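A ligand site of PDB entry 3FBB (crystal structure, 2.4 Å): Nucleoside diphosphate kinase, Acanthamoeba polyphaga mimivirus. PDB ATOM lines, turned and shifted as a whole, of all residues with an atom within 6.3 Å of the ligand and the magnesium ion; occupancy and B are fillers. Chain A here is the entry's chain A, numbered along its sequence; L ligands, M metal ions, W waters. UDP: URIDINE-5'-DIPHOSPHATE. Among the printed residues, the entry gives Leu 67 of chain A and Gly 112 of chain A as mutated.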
ATOM      1  N   LYS A  14     -12.774  16.250   5.755  1.00  0.00           N
ATOM      2  CA  LYS A  14     -13.932  17.115   5.930  1.00  0.00           C
ATOM      3  C   LYS A  14     -13.912  18.326   4.985  1.00  0.00           C
ATOM      4  O   LYS A  14     -12.862  18.635   4.410  1.00  0.00           O
ATOM      5  CB  LYS A  14     -14.059  17.500   7.402  1.00  0.00           C
ATOM      6  CG  LYS A  14     -14.114  16.281   8.307  1.00  0.00           C
ATOM      7  CD  LYS A  14     -14.337  16.692   9.753  1.00  0.00           C
ATOM      8  CE  LYS A  14     -14.530  15.493  10.670  1.00  0.00           C
ATOM      9  NZ  LYS A  14     -14.735  15.915  12.095  1.00  0.00           N
ATOM     10  N   TYR A  55     -22.652   9.858  12.185  1.00  0.00           N
ATOM     11  CA  TYR A  55     -22.592  10.555  13.456  1.00  0.00           C
ATOM     12  C   TYR A  55     -23.814  10.254  14.327  1.00  0.00           C
ATOM     13  O   TYR A  55     -24.259  11.109  15.101  1.00  0.00           O
ATOM     14  CB  TYR A  55     -22.463  12.076  13.245  1.00  0.00           C
ATOM     15  CG  TYR A  55     -21.063  12.499  12.868  1.00  0.00           C
ATOM     16  CD1 TYR A  55     -20.816  13.197  11.678  1.00  0.00           C
ATOM     17  CD2 TYR A  55     -19.986  12.210  13.692  1.00  0.00           C
ATOM     18  CE1 TYR A  55     -19.531  13.584  11.343  1.00  0.00           C
ATOM     19  CE2 TYR A  55     -18.710  12.580  13.358  1.00  0.00           C
ATOM     20  CZ  TYR A  55     -18.482  13.267  12.189  1.00  0.00           C
ATOM     21  OH  TYR A  55     -17.193  13.642  11.865  1.00  0.00           O
ATOM     22  N   HIS A  58     -24.016  10.759  18.019  1.00  0.00           N
ATOM     23  CA  HIS A  58     -24.012  12.158  18.442  1.00  0.00           C
ATOM     24  C   HIS A  58     -25.377  12.798  18.203  1.00  0.00           C
ATOM     25  O   HIS A  58     -25.546  14.005  18.391  1.00  0.00           O
ATOM     26  CB  HIS A  58     -22.949  12.965  17.658  1.00  0.00           C
ATOM     27  CG  HIS A  58     -21.567  12.391  17.729  1.00  0.00           C
ATOM     28  ND1 HIS A  58     -20.556  12.965  18.471  1.00  0.00           N
ATOM     29  CD2 HIS A  58     -21.022  11.304  17.127  1.00  0.00           C
ATOM     30  CE1 HIS A  58     -19.452  12.258  18.327  1.00  0.00           C
ATOM     31  NE2 HIS A  58     -19.704  11.242  17.519  1.00  0.00           N
ATOM     32  N   SER A  62     -26.010  18.917  21.274  1.00  0.00           N
ATOM     33  CA  SER A  62     -26.367  20.257  20.836  1.00  0.00           C
ATOM     34  C   SER A  62     -25.866  20.520  19.422  1.00  0.00           C
ATOM     35  O   SER A  62     -26.538  21.184  18.609  1.00  0.00           O
ATOM     36  CB  SER A  62     -25.772  21.285  21.804  1.00  0.00           C
ATOM     37  OG  SER A  62     -24.528  20.806  22.313  1.00  0.00           O
ATOM     38  N   TYR A  63     -24.693  19.978  19.120  1.00  0.00           N
ATOM     39  CA  TYR A  63     -23.963  20.343  17.913  1.00  0.00           C
ATOM     40  C   TYR A  63     -24.370  19.520  16.705  1.00  0.00           C
ATOM     41  O   TYR A  63     -23.997  19.848  15.582  1.00  0.00           O
ATOM     42  CB  TYR A  63     -22.442  20.267  18.132  1.00  0.00           C
ATOM     43  CG  TYR A  63     -21.961  18.906  18.576  1.00  0.00           C
ATOM     44  CD1 TYR A  63     -21.807  17.864  17.664  1.00  0.00           C
ATOM     45  CD2 TYR A  63     -21.676  18.653  19.914  1.00  0.00           C
ATOM     46  CE1 TYR A  63     -21.379  16.608  18.075  1.00  0.00           C
ATOM     47  CE2 TYR A  63     -21.235  17.401  20.324  1.00  0.00           C
ATOM     48  CZ  TYR A  63     -21.089  16.385  19.399  1.00  0.00           C
ATOM     49  OH  TYR A  63     -20.665  15.142  19.798  1.00  0.00           O
ATOM     50  N   ASP A  66     -25.684  21.401  13.313  1.00  0.00           N
ATOM     51  CA  ASP A  66     -24.657  22.186  12.672  1.00  0.00           C
ATOM     52  C   ASP A  66     -23.531  21.302  12.126  1.00  0.00           C
ATOM     53  O   ASP A  66     -22.912  21.620  11.112  1.00  0.00           O
ATOM     54  CB  ASP A  66     -24.102  23.224  13.648  1.00  0.00           C
ATOM     55  CG  ASP A  66     -25.146  24.276  14.037  1.00  0.00           C
ATOM     56  OD1 ASP A  66     -26.038  24.589  13.196  1.00  0.00           O
ATOM     57  OD2 ASP A  66     -25.060  24.787  15.179  1.00  0.00           O
ATOM     58  N   LEU A  67     -23.284  20.181  12.797  1.00  0.00           N
ATOM     59  CA  LEU A  67     -22.279  19.234  12.334  1.00  0.00           C
ATOM     60  C   LEU A  67     -22.672  18.665  10.977  1.00  0.00           C
ATOM     61  O   LEU A  67     -21.880  18.700  10.022  1.00  0.00           O
ATOM     62  CB  LEU A  67     -22.084  18.095  13.338  1.00  0.00           C
ATOM     63  CG  LEU A  67     -21.156  16.962  12.874  1.00  0.00           C
ATOM     64  CD1 LEU A  67     -19.857  17.526  12.318  1.00  0.00           C
ATOM     65  CD2 LEU A  67     -20.868  15.979  14.014  1.00  0.00           C
ATOM     66  N   PHE A  70     -22.498  21.274   8.245  1.00  0.00           N
ATOM     67  CA  PHE A  70     -21.121  21.456   7.835  1.00  0.00           C
ATOM     68  C   PHE A  70     -20.615  20.275   6.991  1.00  0.00           C
ATOM     69  O   PHE A  70     -20.025  20.466   5.920  1.00  0.00           O
ATOM     70  CB  PHE A  70     -20.242  21.658   9.069  1.00  0.00           C
ATOM     71  CG  PHE A  70     -18.774  21.461   8.807  1.00  0.00           C
ATOM     72  CD1 PHE A  70     -18.108  20.347   9.299  1.00  0.00           C
ATOM     73  CD2 PHE A  70     -18.058  22.396   8.088  1.00  0.00           C
ATOM     74  CE1 PHE A  70     -16.749  20.167   9.072  1.00  0.00           C
ATOM     75  CE2 PHE A  70     -16.694  22.225   7.860  1.00  0.00           C
ATOM     76  CZ  PHE A  70     -16.051  21.111   8.351  1.00  0.00           C
ATOM     77  N   MET A  71     -20.896  19.067   7.453  1.00  0.00           N
ATOM     78  CA  MET A  71     -20.462  17.881   6.738  1.00  0.00           C
ATOM     79  C   MET A  71     -21.046  17.776   5.331  1.00  0.00           C
ATOM     80  O   MET A  71     -20.485  17.079   4.483  1.00  0.00           O
ATOM     81  CB  MET A  71     -20.725  16.620   7.570  1.00  0.00           C
ATOM     82  CG  MET A  71     -19.824  16.501   8.801  1.00  0.00           C
ATOM     83  SD  MET A  71     -18.057  16.413   8.385  1.00  0.00           S
ATOM     84  CE  MET A  71     -17.974  14.846   7.551  1.00  0.00           C
ATOM     85  N   ARG A  91      -5.689   7.363  14.402  1.00  0.00           N
ATOM     86  CA  ARG A  91      -6.343   8.152  15.438  1.00  0.00           C
ATOM     87  C   ARG A  91      -5.378   9.100  16.136  1.00  0.00           C
ATOM     88  O   ARG A  91      -5.677  10.278  16.342  1.00  0.00           O
ATOM     89  CB  ARG A  91      -6.998   7.238  16.469  1.00  0.00           C
ATOM     90  CG  ARG A  91      -8.496   7.362  16.527  1.00  0.00           C
ATOM     91  CD  ARG A  91      -8.859   8.435  17.530  1.00  0.00           C
ATOM     92  NE  ARG A  91     -10.069   9.150  17.166  1.00  0.00           N
ATOM     93  CZ  ARG A  91     -10.848   9.763  18.047  1.00  0.00           C
ATOM     94  NH1 ARG A  91     -10.556   9.709  19.352  1.00  0.00           N
ATOM     95  NH2 ARG A  91     -11.925  10.424  17.644  1.00  0.00           N
ATOM     96  N   GLN A  94      -4.529  11.926  13.762  1.00  0.00           N
ATOM     97  CA  GLN A  94      -5.568  12.932  13.824  1.00  0.00           C
ATOM     98  C   GLN A  94      -5.332  13.857  15.014  1.00  0.00           C
ATOM     99  O   GLN A  94      -5.336  15.081  14.883  1.00  0.00           O
ATOM    100  CB  GLN A  94      -6.938  12.259  13.918  1.00  0.00           C
ATOM    101  CG  GLN A  94      -8.065  13.167  14.361  1.00  0.00           C
ATOM    102  CD  GLN A  94      -9.292  12.388  14.753  1.00  0.00           C
ATOM    103  OE1 GLN A  94     -10.067  11.962  13.911  1.00  0.00           O
ATOM    104  NE2 GLN A  94      -9.474  12.191  16.049  1.00  0.00           N
ATOM    105  N   GLY A  95      -5.114  13.259  16.188  1.00  0.00           N
ATOM    106  CA  GLY A  95      -4.848  14.031  17.387  1.00  0.00           C
ATOM    107  C   GLY A  95      -5.958  15.030  17.689  1.00  0.00           C
ATOM    108  O   GLY A  95      -7.142  14.769  17.419  1.00  0.00           O
ATOM    109  N   ARG A 104      -4.679  17.638  13.371  1.00  0.00           N
ATOM    110  CA  ARG A 104      -5.486  18.666  14.012  1.00  0.00           C
ATOM    111  C   ARG A 104      -4.658  19.655  14.831  1.00  0.00           C
ATOM    112  O   ARG A 104      -4.932  20.867  14.833  1.00  0.00           O
ATOM    113  CB  ARG A 104      -6.544  18.013  14.888  1.00  0.00           C
ATOM    114  CG  ARG A 104      -7.718  17.467  14.098  1.00  0.00           C
ATOM    115  CD  ARG A 104      -8.818  17.003  15.042  1.00  0.00           C
ATOM    116  NE  ARG A 104      -9.839  16.267  14.328  1.00  0.00           N
ATOM    117  CZ  ARG A 104     -10.764  15.539  14.936  1.00  0.00           C
ATOM    118  NH1 ARG A 104     -10.791  15.488  16.261  1.00  0.00           N
ATOM    119  NH2 ARG A 104     -11.658  14.871  14.229  1.00  0.00           N
ATOM    120  N   ASP A 110     -10.549  24.683  15.681  1.00  0.00           N
ATOM    121  CA  ASP A 110     -11.982  24.811  15.912  1.00  0.00           C
ATOM    122  C   ASP A 110     -12.546  23.466  16.311  1.00  0.00           C
ATOM    123  O   ASP A 110     -12.123  22.440  15.778  1.00  0.00           O
ATOM    124  CB  ASP A 110     -12.674  25.292  14.636  1.00  0.00           C
ATOM    125  CG  ASP A 110     -14.131  25.673  14.867  1.00  0.00           C
ATOM    126  OD1 ASP A 110     -15.035  24.894  14.484  1.00  0.00           O
ATOM    127  OD2 ASP A 110     -14.370  26.750  15.430  1.00  0.00           O
ATOM    128  N   ILE A 111     -13.489  23.443  17.250  1.00  0.00           N
ATOM    129  CA  ILE A 111     -14.053  22.172  17.711  1.00  0.00           C
ATOM    130  C   ILE A 111     -14.918  21.478  16.665  1.00  0.00           C
ATOM    131  O   ILE A 111     -15.144  20.282  16.735  1.00  0.00           O
ATOM    132  CB  ILE A 111     -14.888  22.309  19.017  1.00  0.00           C
ATOM    133  CG1 ILE A 111     -15.452  23.727  19.168  1.00  0.00           C
ATOM    134  CG2 ILE A 111     -14.067  21.888  20.231  1.00  0.00           C
ATOM    135  CD1 ILE A 111     -16.664  24.048  18.266  1.00  0.00           C
ATOM    136  N   GLY A 112     -15.402  22.252  15.694  1.00  0.00           N
ATOM    137  CA  GLY A 112     -16.249  21.719  14.640  1.00  0.00           C
ATOM    138  C   GLY A 112     -15.489  21.488  13.352  1.00  0.00           C
ATOM    139  O   GLY A 112     -15.410  20.356  12.850  1.00  0.00           O
ATOM    140  N   GLU A 113     -14.901  22.555  12.815  1.00  0.00           N
ATOM    141  CA  GLU A 113     -14.157  22.451  11.572  1.00  0.00           C
ATOM    142  C   GLU A 113     -12.730  21.978  11.864  1.00  0.00           C
ATOM    143  O   GLU A 113     -11.836  22.766  12.165  1.00  0.00           O
ATOM    144  CB  GLU A 113     -14.184  23.774  10.804  1.00  0.00           C
ATOM    145  CG  GLU A 113     -15.620  24.354  10.731  1.00  0.00           C
ATOM    146  CD  GLU A 113     -15.805  25.337   9.584  1.00  0.00           C
ATOM    147  OE1 GLU A 113     -14.836  25.547   8.826  1.00  0.00           O
ATOM    148  OE2 GLU A 113     -16.925  25.899   9.443  1.00  0.00           O
ATOM    149  N   ASN A 114     -12.541  20.677  11.768  1.00  0.00           N
ATOM    150  CA  ASN A 114     -11.299  20.078  12.210  1.00  0.00           C
ATOM    151  C   ASN A 114     -10.729  19.077  11.226  1.00  0.00           C
ATOM    152  O   ASN A 114     -10.018  18.155  11.607  1.00  0.00           O
ATOM    153  CB  ASN A 114     -11.452  19.488  13.623  1.00  0.00           C
ATOM    154  CG  ASN A 114     -12.529  18.425  13.700  1.00  0.00           C
ATOM    155  OD1 ASN A 114     -12.991  17.914  12.687  1.00  0.00           O
ATOM    156  ND2 ASN A 114     -12.914  18.068  14.917  1.00  0.00           N
ATOM    157  N   ILE A 116     -10.524  16.352   9.633  1.00  0.00           N
ATOM    158  CA  ILE A 116     -10.484  14.909   9.469  1.00  0.00           C
ATOM    159  C   ILE A 116     -11.261  14.109  10.513  1.00  0.00           C
ATOM    160  O   ILE A 116     -11.218  14.418  11.697  1.00  0.00           O
ATOM    161  CB  ILE A 116      -9.008  14.415   9.483  1.00  0.00           C
ATOM    162  CG1 ILE A 116      -8.927  12.907   9.468  1.00  0.00           C
ATOM    163  CG2 ILE A 116      -8.265  14.973  10.681  1.00  0.00           C
ATOM    164  CD1 ILE A 116      -7.513  12.396   9.311  1.00  0.00           C
ATOM    165  N   HIS A 117     -11.979  13.074  10.075  1.00  0.00           N
ATOM    166  CA  HIS A 117     -12.467  12.046  10.984  1.00  0.00           C
ATOM    167  C   HIS A 117     -11.675  10.752  10.816  1.00  0.00           C
ATOM    168  O   HIS A 117     -11.410  10.326   9.685  1.00  0.00           O
ATOM    169  CB  HIS A 117     -13.963  11.767  10.786  1.00  0.00           C
ATOM    170  CG  HIS A 117     -14.405  10.483  11.443  1.00  0.00           C
ATOM    171  ND1 HIS A 117     -15.036  10.455  12.665  1.00  0.00           N
ATOM    172  CD2 HIS A 117     -14.242   9.191  11.064  1.00  0.00           C
ATOM    173  CE1 HIS A 117     -15.264   9.195  13.004  1.00  0.00           C
ATOM    174  NE2 HIS A 117     -14.797   8.413  12.052  1.00  0.00           N
ATOM    175  N   ALA A 118     -11.313  10.140  11.946  1.00  0.00           N
ATOM    176  CA  ALA A 118     -10.744   8.778  11.940  1.00  0.00           C
ATOM    177  C   ALA A 118     -11.561   7.887  12.892  1.00  0.00           C
ATOM    178  O   ALA A 118     -11.992   8.350  13.943  1.00  0.00           O
ATOM    179  CB  ALA A 118      -9.281   8.800  12.368  1.00  0.00           C
ATOM    180  N   ASP A 120     -12.384   5.376  15.824  1.00  0.00           N
ATOM    181  CA  ASP A 120     -11.724   5.326  17.111  1.00  0.00           C
ATOM    182  C   ASP A 120     -11.722   3.963  17.802  1.00  0.00           C
ATOM    183  O   ASP A 120     -11.214   3.852  18.908  1.00  0.00           O
ATOM    184  CB  ASP A 120     -12.291   6.390  18.057  1.00  0.00           C
ATOM    185  CG  ASP A 120     -13.708   6.073  18.501  1.00  0.00           C
ATOM    186  OD1 ASP A 120     -14.277   5.057  18.036  1.00  0.00           O
ATOM    187  OD2 ASP A 120     -14.248   6.848  19.331  1.00  0.00           O
HETATM  188  N1  UDP L   1     -18.139  18.501  17.025  1.00  0.00           N
HETATM  189  C2  UDP L   1     -18.658  19.795  16.959  1.00  0.00           C
HETATM  190  N3  UDP L   1     -18.866  20.524  18.117  1.00  0.00           N
HETATM  191  C4  UDP L   1     -18.555  19.959  19.331  1.00  0.00           C
HETATM  192  C5  UDP L   1     -18.027  18.660  19.397  1.00  0.00           C
HETATM  193  C6  UDP L   1     -17.723  17.981  18.226  1.00  0.00           C
HETATM  194  O2  UDP L   1     -18.949  20.315  15.873  1.00  0.00           O
HETATM  195  O4  UDP L   1     -18.733  20.612  20.347  1.00  0.00           O
HETATM  196  C1' UDP L   1     -17.932  17.751  15.758  1.00  0.00           C
HETATM  197  C2' UDP L   1     -16.442  17.751  15.414  1.00  0.00           C
HETATM  198  O2' UDP L   1     -16.279  17.986  14.042  1.00  0.00           O
HETATM  199  C3' UDP L   1     -15.977  16.368  15.780  1.00  0.00           C
HETATM  200  C4' UDP L   1     -17.251  15.519  15.665  1.00  0.00           C
HETATM  201  O4' UDP L   1     -18.339  16.395  15.871  1.00  0.00           O
HETATM  202  O3' UDP L   1     -14.962  15.904  14.930  1.00  0.00           O
HETATM  203  C5' UDP L   1     -17.290  14.395  16.690  1.00  0.00           C
HETATM  204  O5' UDP L   1     -17.068  14.948  17.973  1.00  0.00           O
HETATM  205  PA  UDP L   1     -15.906  14.325  18.888  1.00  0.00           P
HETATM  206  O1A UDP L   1     -16.094  12.856  19.061  1.00  0.00           O
HETATM  207  O2A UDP L   1     -15.831  15.095  20.171  1.00  0.00           O
HETATM  208  O3A UDP L   1     -14.567  14.655  18.027  1.00  0.00           O
HETATM  209  PB  UDP L   1     -13.581  13.570  17.338  1.00  0.00           P
HETATM  210  O1B UDP L   1     -12.205  13.835  17.775  1.00  0.00           O
HETATM  211  O2B UDP L   1     -13.785  13.675  15.869  1.00  0.00           O
HETATM  212  O3B UDP L   1     -13.909  12.176  17.730  1.00  0.00           O
HETATM  213 MG    MG M   1     -15.259  10.352  18.793  1.00  0.00          MG
HETATM  214  O   HOH W   1     -15.938  11.055  16.474  1.00  0.00           O
HETATM  215  O   HOH W   2     -15.267  13.334  13.474  1.00  0.00           O
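An oxygen (O1B) of the ligand lies within salt-bridge range of the guanidinium group (NH2) of Arg 91.
The guanidinium group (NH1) of Arg 104 lies within salt-bridge range of an oxygen (O1B) of the ligand (2.7 Å).
The backbone carbonyl oxygen (O) of Gly 112 sits at hydrogen-bond distance from an oxygen (O2') of the ligand.
An oxygen (O3') of the ligand lies within hydrogen-bond range of the side-chain amino group of Lys 14 (2.8 Å).
The side-chain amide nitrogen (ND2) of Asn 114 lies within hydrogen-bond range of an oxygen (O3') of the ligand (3.0 Å).
The guanidinium group (NE) of Arg 91 sits close to the side-chain amide nitrogen (NE2) of Gln 94 (3.3 Å).
NE of Arg 104 is in hydrogen-bond range of O of Asn 114.
The backbone carbonyl oxygen (O) of Gln 94 sits at hydrogen-bond distance from the backbone NH (N) of Arg 104, at 3.0 Å.
The guanidinium group of Arg 104 sits at hydrogen-bond distance from the backbone carbonyl oxygen of Ile 116 (2.6 Å).
OD1 of Asn 114 lies close to O of Gly 112 (3.4 Å).
N of Gly 112 is in hydrogen-bond range of OD1 of Asp 110 (2.9 Å).
OH of Tyr 55 is in hydrogen-bond range of NZ of Lys 14 (3.4 Å).
OH of Tyr 63 lies within hydrogen-bond range of ND1 of His 58, at 2.6 Å.
N1 of the ligand lies close to O of Ile 111, 3.5 Å away.
His 58 touches the ligand (CE1 to C5', 3.5 Å).
CD2 of Tyr 63 touches C4 of the ligand, at 3.4 Å.
Leu 67 touches the ligand.
Gln 94 touches the ligand (NE2 to O1B, 3.6 Å).
Hydrophobic or aromatic side chains within 4 Å of the ligand: His 58, Tyr 63 and Leu 67.
Of the 22 residues printed, 10 come within 4 Å of the ligand.
Arg 91 touches the magnesium ion.
Asp 120 touches the magnesium ion.
Of the 22 residues printed, 2 come within 4 Å of the magnesium ion.
The nearest printed residue that does not touch the magnesium ion is His 58 (4.6 Å).
The magnesium ion is bound by an oxygen (O3B) of the ligand (2.5 Å) and water W1 (2.5 Å).
Slightly farther from the magnesium ion lies an oxygen (O1A) of the ligand (2.7 Å).
Water W2 lies within hydrogen-bond range of the side-chain hydroxyl (OH) of Tyr 55, an oxygen (O2B) of the ligand, the side-chain amino group (NZ) of Lys 14 and a ring nitrogen (ND1) of His 117.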
